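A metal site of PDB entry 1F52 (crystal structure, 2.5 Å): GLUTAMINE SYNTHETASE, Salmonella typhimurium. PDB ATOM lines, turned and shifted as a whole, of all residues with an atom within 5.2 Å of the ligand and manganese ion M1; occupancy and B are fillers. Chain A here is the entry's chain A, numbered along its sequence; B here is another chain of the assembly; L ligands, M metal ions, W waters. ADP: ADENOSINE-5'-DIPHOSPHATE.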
ATOM      1  N   LEU A 125      19.354  13.639   8.656  1.00  0.00           N
ATOM      2  CA  LEU A 125      18.434  13.467   7.548  1.00  0.00           C
ATOM      3  C   LEU A 125      18.796  12.326   6.626  1.00  0.00           C
ATOM      4  O   LEU A 125      19.918  12.265   6.098  1.00  0.00           O
ATOM      5  CB  LEU A 125      18.316  14.766   6.772  1.00  0.00           C
ATOM      6  CG  LEU A 125      17.161  15.687   7.169  1.00  0.00           C
ATOM      7  CD1 LEU A 125      16.724  15.461   8.604  1.00  0.00           C
ATOM      8  CD2 LEU A 125      17.582  17.103   6.930  1.00  0.00           C
ATOM      9  N   PHE A 126      17.852  11.405   6.439  1.00  0.00           N
ATOM     10  CA  PHE A 126      18.037  10.245   5.572  1.00  0.00           C
ATOM     11  C   PHE A 126      17.065  10.203   4.422  1.00  0.00           C
ATOM     12  O   PHE A 126      15.841  10.345   4.603  1.00  0.00           O
ATOM     13  CB  PHE A 126      17.903   8.955   6.364  1.00  0.00           C
ATOM     14  CG  PHE A 126      19.194   8.484   6.945  1.00  0.00           C
ATOM     15  CD1 PHE A 126      19.681   9.023   8.125  1.00  0.00           C
ATOM     16  CD2 PHE A 126      19.932   7.479   6.312  1.00  0.00           C
ATOM     17  CE1 PHE A 126      20.881   8.578   8.675  1.00  0.00           C
ATOM     18  CE2 PHE A 126      21.132   7.028   6.845  1.00  0.00           C
ATOM     19  CZ  PHE A 126      21.605   7.572   8.023  1.00  0.00           C
ATOM     20  N   GLY A 127      17.615  10.022   3.232  1.00  0.00           N
ATOM     21  CA  GLY A 127      16.811   9.916   2.036  1.00  0.00           C
ATOM     22  C   GLY A 127      17.237   8.674   1.277  1.00  0.00           C
ATOM     23  O   GLY A 127      18.049   8.764   0.349  1.00  0.00           O
ATOM     24  N   PRO A 128      16.771   7.488   1.695  1.00  0.00           N
ATOM     25  CA  PRO A 128      17.135   6.241   1.017  1.00  0.00           C
ATOM     26  C   PRO A 128      16.305   6.032  -0.249  1.00  0.00           C
ATOM     27  O   PRO A 128      15.182   6.518  -0.352  1.00  0.00           O
ATOM     28  CB  PRO A 128      16.842   5.201   2.078  1.00  0.00           C
ATOM     29  CG  PRO A 128      15.639   5.751   2.753  1.00  0.00           C
ATOM     30  CD  PRO A 128      15.943   7.225   2.881  1.00  0.00           C
ATOM     31  N   GLU A 129      16.881   5.340  -1.227  1.00  0.00           N
ATOM     32  CA  GLU A 129      16.208   5.097  -2.501  1.00  0.00           C
ATOM     33  C   GLU A 129      16.129   3.604  -2.773  1.00  0.00           C
ATOM     34  O   GLU A 129      16.884   3.064  -3.579  1.00  0.00           O
ATOM     35  CB  GLU A 129      16.991   5.779  -3.630  1.00  0.00           C
ATOM     36  CG  GLU A 129      17.316   7.230  -3.323  1.00  0.00           C
ATOM     37  CD  GLU A 129      18.234   7.895  -4.337  1.00  0.00           C
ATOM     38  OE1 GLU A 129      17.845   9.000  -4.757  1.00  0.00           O
ATOM     39  OE2 GLU A 129      19.305   7.363  -4.697  1.00  0.00           O
ATOM     40  N   GLU A 207       8.105  11.523  -4.293  1.00  0.00           N
ATOM     41  CA  GLU A 207       8.729  12.480  -5.189  1.00  0.00           C
ATOM     42  C   GLU A 207       8.664  12.042  -6.646  1.00  0.00           C
ATOM     43  O   GLU A 207       8.554  12.872  -7.547  1.00  0.00           O
ATOM     44  CB  GLU A 207      10.155  12.781  -4.749  1.00  0.00           C
ATOM     45  CG  GLU A 207      10.166  13.391  -3.358  1.00  0.00           C
ATOM     46  CD  GLU A 207      11.520  13.892  -2.915  1.00  0.00           C
ATOM     47  OE1 GLU A 207      12.519  13.209  -3.220  1.00  0.00           O
ATOM     48  OE2 GLU A 207      11.595  14.962  -2.281  1.00  0.00           O
ATOM     49  N   GLU A 220      10.972   1.531  -9.160  1.00  0.00           N
ATOM     50  CA  GLU A 220      11.363   2.370  -8.025  1.00  0.00           C
ATOM     51  C   GLU A 220      10.367   3.471  -7.717  1.00  0.00           C
ATOM     52  O   GLU A 220       9.881   4.152  -8.620  1.00  0.00           O
ATOM     53  CB  GLU A 220      12.764   3.000  -8.234  1.00  0.00           C
ATOM     54  CG  GLU A 220      13.258   3.875  -7.087  1.00  0.00           C
ATOM     55  CD  GLU A 220      14.661   4.400  -7.271  1.00  0.00           C
ATOM     56  OE1 GLU A 220      15.319   4.047  -8.263  1.00  0.00           O
ATOM     57  OE2 GLU A 220      15.105   5.195  -6.410  1.00  0.00           O
ATOM     58  N   ALA A 222      10.369   6.804  -5.426  1.00  0.00           N
ATOM     59  CA  ALA A 222      11.208   7.708  -4.666  1.00  0.00           C
ATOM     60  C   ALA A 222      10.397   8.525  -3.694  1.00  0.00           C
ATOM     61  O   ALA A 222       9.427   9.177  -4.068  1.00  0.00           O
ATOM     62  CB  ALA A 222      11.979   8.627  -5.612  1.00  0.00           C
ATOM     63  N   THR A 223      10.792   8.465  -2.437  1.00  0.00           N
ATOM     64  CA  THR A 223      10.095   9.191  -1.388  1.00  0.00           C
ATOM     65  C   THR A 223      10.979  10.279  -0.759  1.00  0.00           C
ATOM     66  O   THR A 223      12.204  10.171  -0.785  1.00  0.00           O
ATOM     67  CB  THR A 223       9.617   8.246  -0.295  1.00  0.00           C
ATOM     68  OG1 THR A 223      10.729   7.532   0.233  1.00  0.00           O
ATOM     69  CG2 THR A 223       8.602   7.264  -0.864  1.00  0.00           C
ATOM     70  N   ARG A 224      10.350  11.316  -0.199  1.00  0.00           N
ATOM     71  CA  ARG A 224      11.066  12.399   0.461  1.00  0.00           C
ATOM     72  C   ARG A 224      11.735  11.904   1.727  1.00  0.00           C
ATOM     73  O   ARG A 224      11.227  11.048   2.433  1.00  0.00           O
ATOM     74  CB  ARG A 224      10.124  13.560   0.763  1.00  0.00           C
ATOM     75  CG  ARG A 224      10.830  14.822   1.242  1.00  0.00           C
ATOM     76  CD  ARG A 224       9.898  15.724   2.033  1.00  0.00           C
ATOM     77  NE  ARG A 224       9.326  15.043   3.185  1.00  0.00           N
ATOM     78  CZ  ARG A 224       8.745  15.658   4.201  1.00  0.00           C
ATOM     79  NH1 ARG A 224       8.655  16.987   4.213  1.00  0.00           N
ATOM     80  NH2 ARG A 224       8.252  14.963   5.215  1.00  0.00           N
ATOM     81  N   PHE A 225      12.905  12.500   1.984  1.00  0.00           N
ATOM     82  CA  PHE A 225      13.714  12.153   3.148  1.00  0.00           C
ATOM     83  C   PHE A 225      12.907  12.487   4.388  1.00  0.00           C
ATOM     84  O   PHE A 225      11.795  12.988   4.298  1.00  0.00           O
ATOM     85  CB  PHE A 225      15.006  13.014   3.179  1.00  0.00           C
ATOM     86  CG  PHE A 225      14.649  14.460   3.400  1.00  0.00           C
ATOM     87  CD1 PHE A 225      14.357  15.275   2.321  1.00  0.00           C
ATOM     88  CD2 PHE A 225      14.545  15.000   4.681  1.00  0.00           C
ATOM     89  CE1 PHE A 225      13.947  16.585   2.516  1.00  0.00           C
ATOM     90  CE2 PHE A 225      14.140  16.309   4.888  1.00  0.00           C
ATOM     91  CZ  PHE A 225      13.834  17.104   3.805  1.00  0.00           C
ATOM     92  N   HIS A 269      20.474   3.541  -2.279  1.00  0.00           N
ATOM     93  CA  HIS A 269      21.341   4.676  -2.031  1.00  0.00           C
ATOM     94  C   HIS A 269      20.817   5.440  -0.845  1.00  0.00           C
ATOM     95  O   HIS A 269      19.608   5.594  -0.675  1.00  0.00           O
ATOM     96  CB  HIS A 269      21.303   5.634  -3.209  1.00  0.00           C
ATOM     97  CG  HIS A 269      21.794   5.067  -4.489  1.00  0.00           C
ATOM     98  ND1 HIS A 269      21.639   5.716  -5.697  1.00  0.00           N
ATOM     99  CD2 HIS A 269      22.469   3.914  -4.769  1.00  0.00           C
ATOM    100  CE1 HIS A 269      22.186   4.998  -6.653  1.00  0.00           C
ATOM    101  NE2 HIS A 269      22.697   3.905  -6.117  1.00  0.00           N
ATOM    102  N   HIS A 271      21.003   9.119   0.951  1.00  0.00           N
ATOM    103  CA  HIS A 271      21.366  10.519   0.973  1.00  0.00           C
ATOM    104  C   HIS A 271      21.321  10.912   2.434  1.00  0.00           C
ATOM    105  O   HIS A 271      20.377  10.552   3.152  1.00  0.00           O
ATOM    106  CB  HIS A 271      20.362  11.341   0.184  1.00  0.00           C
ATOM    107  CG  HIS A 271      20.415  11.131  -1.290  1.00  0.00           C
ATOM    108  ND1 HIS A 271      20.472  12.164  -2.190  1.00  0.00           N
ATOM    109  CD2 HIS A 271      20.436   9.998  -2.034  1.00  0.00           C
ATOM    110  CE1 HIS A 271      20.528  11.686  -3.416  1.00  0.00           C
ATOM    111  NE2 HIS A 271      20.511  10.374  -3.350  1.00  0.00           N
ATOM    112  N   MET A 272      22.357  11.612   2.896  1.00  0.00           N
ATOM    113  CA  MET A 272      22.419  12.049   4.278  1.00  0.00           C
ATOM    114  C   MET A 272      22.944  13.471   4.426  1.00  0.00           C
ATOM    115  O   MET A 272      23.657  13.982   3.560  1.00  0.00           O
ATOM    116  CB  MET A 272      23.321  11.123   5.077  1.00  0.00           C
ATOM    117  CG  MET A 272      22.791   9.728   5.237  1.00  0.00           C
ATOM    118  SD  MET A 272      24.075   8.674   5.852  1.00  0.00           S
ATOM    119  CE  MET A 272      25.198   8.719   4.480  1.00  0.00           C
ATOM    120  N   SER A 273      22.596  14.099   5.540  1.00  0.00           N
ATOM    121  CA  SER A 273      23.023  15.445   5.874  1.00  0.00           C
ATOM    122  C   SER A 273      22.653  15.675   7.321  1.00  0.00           C
ATOM    123  O   SER A 273      21.769  14.999   7.852  1.00  0.00           O
ATOM    124  CB  SER A 273      22.349  16.493   4.991  1.00  0.00           C
ATOM    125  OG  SER A 273      20.986  16.640   5.329  1.00  0.00           O
ATOM    126  N   ASN A 280      21.688  23.815   7.484  1.00  0.00           N
ATOM    127  CA  ASN A 280      22.334  22.601   6.973  1.00  0.00           C
ATOM    128  C   ASN A 280      23.829  22.558   7.250  1.00  0.00           C
ATOM    129  O   ASN A 280      24.635  23.104   6.490  1.00  0.00           O
ATOM    130  CB  ASN A 280      22.062  22.468   5.467  1.00  0.00           C
ATOM    131  CG  ASN A 280      22.470  21.108   4.912  1.00  0.00           C
ATOM    132  OD1 ASN A 280      23.281  20.378   5.510  1.00  0.00           O
ATOM    133  ND2 ASN A 280      21.910  20.757   3.766  1.00  0.00           N
ATOM    134  N   ARG A 339      30.702   7.986 -11.219  1.00  0.00           N
ATOM    135  CA  ARG A 339      29.754   7.027 -10.660  1.00  0.00           C
ATOM    136  C   ARG A 339      30.368   5.641 -10.513  1.00  0.00           C
ATOM    137  O   ARG A 339      29.761   4.628 -10.856  1.00  0.00           O
ATOM    138  CB  ARG A 339      28.405   7.017 -11.412  1.00  0.00           C
ATOM    139  CG  ARG A 339      27.447   8.161 -11.015  1.00  0.00           C
ATOM    140  CD  ARG A 339      26.036   7.932 -11.565  1.00  0.00           C
ATOM    141  NE  ARG A 339      25.140   9.096 -11.438  1.00  0.00           N
ATOM    142  CZ  ARG A 339      23.853   9.043 -11.090  1.00  0.00           C
ATOM    143  NH1 ARG A 339      23.100  10.140 -11.008  1.00  0.00           N
ATOM    144  NH2 ARG A 339      23.295   7.871 -10.773  1.00  0.00           N
ATOM    145  N   ARG A 344      28.567   9.629  -3.828  1.00  0.00           N
ATOM    146  CA  ARG A 344      28.339  10.712  -4.786  1.00  0.00           C
ATOM    147  C   ARG A 344      27.996  11.978  -4.053  1.00  0.00           C
ATOM    148  O   ARG A 344      27.369  11.957  -2.988  1.00  0.00           O
ATOM    149  CB  ARG A 344      27.221  10.481  -5.798  1.00  0.00           C
ATOM    150  CG  ARG A 344      27.283  11.538  -6.902  1.00  0.00           C
ATOM    151  CD  ARG A 344      26.421  11.158  -8.086  1.00  0.00           C
ATOM    152  NE  ARG A 344      25.070  10.872  -7.643  1.00  0.00           N
ATOM    153  CZ  ARG A 344      24.162  11.738  -7.243  1.00  0.00           C
ATOM    154  NH1 ARG A 344      24.459  13.033  -7.247  1.00  0.00           N
ATOM    155  NH2 ARG A 344      22.975  11.322  -6.837  1.00  0.00           N
ATOM    156  N   LYS A 352      20.879  24.762   1.031  1.00  0.00           N
ATOM    157  CA  LYS A 352      19.984  24.137   2.003  1.00  0.00           C
ATOM    158  C   LYS A 352      19.812  22.654   1.713  1.00  0.00           C
ATOM    159  O   LYS A 352      19.470  21.875   2.603  1.00  0.00           O
ATOM    160  CB  LYS A 352      18.620  24.838   1.982  1.00  0.00           C
ATOM    161  CG  LYS A 352      18.665  26.298   2.430  1.00  0.00           C
ATOM    162  CD  LYS A 352      17.292  26.930   2.449  1.00  0.00           C
ATOM    163  CE  LYS A 352      17.372  28.377   2.928  1.00  0.00           C
ATOM    164  NZ  LYS A 352      16.057  29.054   2.886  1.00  0.00           N
ATOM    165  N   ALA A 353      20.103  22.266   0.473  1.00  0.00           N
ATOM    166  CA  ALA A 353      19.965  20.884   0.022  1.00  0.00           C
ATOM    167  C   ALA A 353      21.289  20.137  -0.182  1.00  0.00           C
ATOM    168  O   ALA A 353      21.303  19.065  -0.795  1.00  0.00           O
ATOM    169  CB  ALA A 353      19.141  20.846  -1.264  1.00  0.00           C
ATOM    170  N   ARG A 354      22.389  20.679   0.321  1.00  0.00           N
ATOM    171  CA  ARG A 354      23.702  20.037   0.186  1.00  0.00           C
ATOM    172  C   ARG A 354      23.709  18.770   1.059  1.00  0.00           C
ATOM    173  O   ARG A 354      23.269  18.798   2.214  1.00  0.00           O
ATOM    174  CB  ARG A 354      24.801  21.010   0.648  1.00  0.00           C
ATOM    175  CG  ARG A 354      26.128  20.898  -0.112  1.00  0.00           C
ATOM    176  CD  ARG A 354      26.122  21.668  -1.436  1.00  0.00           C
ATOM    177  NE  ARG A 354      26.229  23.112  -1.255  1.00  0.00           N
ATOM    178  CZ  ARG A 354      25.874  24.015  -2.172  1.00  0.00           C
ATOM    179  NH1 ARG A 354      26.007  25.315  -1.919  1.00  0.00           N
ATOM    180  NH2 ARG A 354      25.377  23.622  -3.331  1.00  0.00           N
ATOM    181  N   ARG A 355      24.235  17.674   0.522  1.00  0.00           N
ATOM    182  CA  ARG A 355      24.262  16.389   1.234  1.00  0.00           C
ATOM    183  C   ARG A 355      25.188  15.375   0.545  1.00  0.00           C
ATOM    184  O   ARG A 355      25.754  15.672  -0.504  1.00  0.00           O
ATOM    185  CB  ARG A 355      22.841  15.824   1.216  1.00  0.00           C
ATOM    186  CG  ARG A 355      22.370  15.539  -0.212  1.00  0.00           C
ATOM    187  CD  ARG A 355      20.865  15.600  -0.347  1.00  0.00           C
ATOM    188  NE  ARG A 355      20.447  15.156  -1.677  1.00  0.00           N
ATOM    189  CZ  ARG A 355      19.836  15.915  -2.570  1.00  0.00           C
ATOM    190  NH1 ARG A 355      19.498  15.407  -3.747  1.00  0.00           N
ATOM    191  NH2 ARG A 355      19.552  17.186  -2.313  1.00  0.00           N
ATOM    192  N   GLU A 357      25.656  11.169  -0.852  1.00  0.00           N
ATOM    193  CA  GLU A 357      24.907   9.974  -1.210  1.00  0.00           C
ATOM    194  C   GLU A 357      25.779   8.737  -1.132  1.00  0.00           C
ATOM    195  O   GLU A 357      26.685   8.560  -1.936  1.00  0.00           O
ATOM    196  CB  GLU A 357      24.335  10.079  -2.632  1.00  0.00           C
ATOM    197  CG  GLU A 357      23.476   8.883  -2.972  1.00  0.00           C
ATOM    198  CD  GLU A 357      23.105   8.770  -4.432  1.00  0.00           C
ATOM    199  OE1 GLU A 357      23.987   8.940  -5.285  1.00  0.00           O
ATOM    200  OE2 GLU A 357      21.945   8.452  -4.728  1.00  0.00           O
ATOM    201  N   ARG A 359      26.173   5.183  -1.844  1.00  0.00           N
ATOM    202  CA  ARG A 359      25.551   4.299  -2.803  1.00  0.00           C
ATOM    203  C   ARG A 359      25.556   2.772  -2.572  1.00  0.00           C
ATOM    204  O   ARG A 359      24.814   2.062  -3.255  1.00  0.00           O
ATOM    205  CB  ARG A 359      26.254   4.569  -4.132  1.00  0.00           C
ATOM    206  CG  ARG A 359      26.742   5.972  -4.389  1.00  0.00           C
ATOM    207  CD  ARG A 359      25.716   6.628  -5.273  1.00  0.00           C
ATOM    208  NE  ARG A 359      25.688   5.995  -6.562  1.00  0.00           N
ATOM    209  CZ  ARG A 359      24.944   6.488  -7.529  1.00  0.00           C
ATOM    210  NH1 ARG A 359      24.242   7.582  -7.306  1.00  0.00           N
ATOM    211  NH2 ARG A 359      24.879   5.884  -8.717  1.00  0.00           N
ATOM    212  N   MET B  48      16.095  17.245 -11.985  1.00  0.00           N
ATOM    213  CA  MET B  48      17.363  16.561 -12.260  1.00  0.00           C
ATOM    214  C   MET B  48      17.204  15.069 -12.465  1.00  0.00           C
ATOM    215  O   MET B  48      16.383  14.415 -11.811  1.00  0.00           O
ATOM    216  CB  MET B  48      18.319  16.758 -11.086  1.00  0.00           C
ATOM    217  CG  MET B  48      18.846  18.160 -10.949  1.00  0.00           C
ATOM    218  SD  MET B  48      19.954  18.544 -12.299  1.00  0.00           S
ATOM    219  CE  MET B  48      21.516  18.166 -11.533  1.00  0.00           C
HETATM  220  PB  ADP L   1      19.091   9.936  -7.319  1.00  0.00           P
HETATM  221  O1B ADP L   1      19.055  10.326  -8.805  1.00  0.00           O
HETATM  222  O2B ADP L   1      20.416  10.009  -6.649  1.00  0.00           O
HETATM  223  O3B ADP L   1      18.404   8.414  -7.184  1.00  0.00           O
HETATM  224  PA  ADP L   1      16.306  11.102  -6.422  1.00  0.00           P
HETATM  225  O1A ADP L   1      15.597  11.670  -7.650  1.00  0.00           O
HETATM  226  O2A ADP L   1      15.694   9.692  -6.082  1.00  0.00           O
HETATM  227  O3A ADP L   1      17.981  10.970  -6.629  1.00  0.00           O
HETATM  228  O5' ADP L   1      15.907  12.140  -5.196  1.00  0.00           O
HETATM  229  C5' ADP L   1      15.609  12.089  -3.837  1.00  0.00           C
HETATM  230  C4' ADP L   1      16.350  11.856  -2.559  1.00  0.00           C
HETATM  231  O4' ADP L   1      17.334  12.942  -1.989  1.00  0.00           O
HETATM  232  C3' ADP L   1      15.230  11.888  -1.618  1.00  0.00           C
HETATM  233  O3' ADP L   1      15.353  10.742  -0.812  1.00  0.00           O
HETATM  234  C2' ADP L   1      15.449  13.293  -0.976  1.00  0.00           C
HETATM  235  O2' ADP L   1      14.443  13.554  -0.028  1.00  0.00           O
HETATM  236  C1' ADP L   1      16.841  12.984  -0.541  1.00  0.00           C
HETATM  237  N9  ADP L   1      17.528  14.014   0.577  1.00  0.00           N
HETATM  238  C8  ADP L   1      18.330  13.589   1.704  1.00  0.00           C
HETATM  239  N7  ADP L   1      18.817  14.497   2.563  1.00  0.00           N
HETATM  240  C5  ADP L   1      18.354  15.651   1.972  1.00  0.00           C
HETATM  241  C6  ADP L   1      18.542  16.976   2.359  1.00  0.00           C
HETATM  242  N6  ADP L   1      19.186  17.181   3.367  1.00  0.00           N
HETATM  243  N1  ADP L   1      17.994  17.993   1.654  1.00  0.00           N
HETATM  244  C2  ADP L   1      17.278  17.708   0.534  1.00  0.00           C
HETATM  245  N3  ADP L   1      16.990  16.473  -0.011  1.00  0.00           N
HETATM  246  C4  ADP L   1      17.580  15.435   0.759  1.00  0.00           C
HETATM  247 MN    MN M   1      20.592   7.675  -6.264  1.00  0.00          MN
HETATM  248 MN    MN M   2      17.273   4.089  -9.006  1.00  0.00          MN
HETATM  249  O   HOH W   1      21.744   8.357  -7.898  1.00  0.00           O
HETATM  250  O   HOH W   2      13.882   8.650   1.055  1.00  0.00           O
HETATM  251  O   HOH W   3      19.227   6.359  -8.145  1.00  0.00           O
HETATM  252  O   HOH W   4      15.757   7.445  -8.370  1.00  0.00           O
HETATM  253  O   HOH W   5      19.176  13.063  -9.645  1.00  0.00           O
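Residues that only touch the ligand: Leu 125, Gly 127, Glu 207, Ala 222, Arg 224, Ala 353 and Arg 355.
Hydrophobic or aromatic side chains that line the ligand: Leu 125, Ala 222, Phe 225 and His 271.
Of the 25 residues printed, 14 come within 4 Å of the ligand.
The nearest printed residue that does not touch the ligand is Pro 128 (4.3 Å).
Manganese ion M1 is bound by OE2 of Glu 129, water W1, OE2 of Glu 357, ND1 of His 269, O2B of the ligand, O3B of the ligand and water W3.
His 271 touches manganese ion M1.
NH1 of Arg 359 touches manganese ion M1 (3.8 Å).
Of the 25 residues printed, 5 come within 4 Å of manganese ion M1.
The nearest printed residue that does not touch manganese ion M1 is Arg 344 (4.4 Å).
Water W4 lies within hydrogen-bond range of the side-chain carboxylate of Glu 220 and an oxygen (O2A) of the ligand.
Water W2 lies within hydrogen-bond range of O of Pro 128 (2.9 Å), O of Thr 223 (2.9 Å) and O3' of the ligand (3.2 Å).
OG of Ser 273 sits at hydrogen-bond distance from N6 of the ligand (2.7 Å).
The backbone NH of Phe 225 lies within hydrogen-bond range of an oxygen (O2') of the ligand (2.7 Å).
The guanidinium group (NH2) of Arg 344 lies close to an oxygen (O2B) of the ligand.
An oxygen (O3') of the ligand lies within hydrogen-bond range of the backbone carbonyl oxygen (O) of Thr 223, 3.2 Å away.
O4' of the ligand is in hydrogen-bond range of ND1 of His 271, at 3.2 Å.
A ring nitrogen (NE2) of His 271 sits at hydrogen-bond distance from the side-chain carboxylate (OE1) of Glu 129, 3.3 Å away.
OE1 of Glu 357 is in salt-bridge range of NH2 of Arg 344 (3.0 Å).
The side-chain carboxylate of Glu 357 lies close to a ring nitrogen (NE2) of His 271 (2.8 Å).
OE1 of Glu 357 is in salt-bridge range of NH1 of Arg 359.
N of Leu 125 lies within hydrogen-bond range of O of Ser 273 (2.9 Å).
The backbone NH of Gly 127 lies within hydrogen-bond range of the backbone carbonyl oxygen of His 271 (2.8 Å).
The backbone NH of Glu 207 lies within hydrogen-bond range of the backbone carbonyl oxygen of Ala 222.
The guanidinium group of Arg 355 lies within hydrogen-bond range of the backbone carbonyl oxygen of Ala 353 (3.0 Å).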
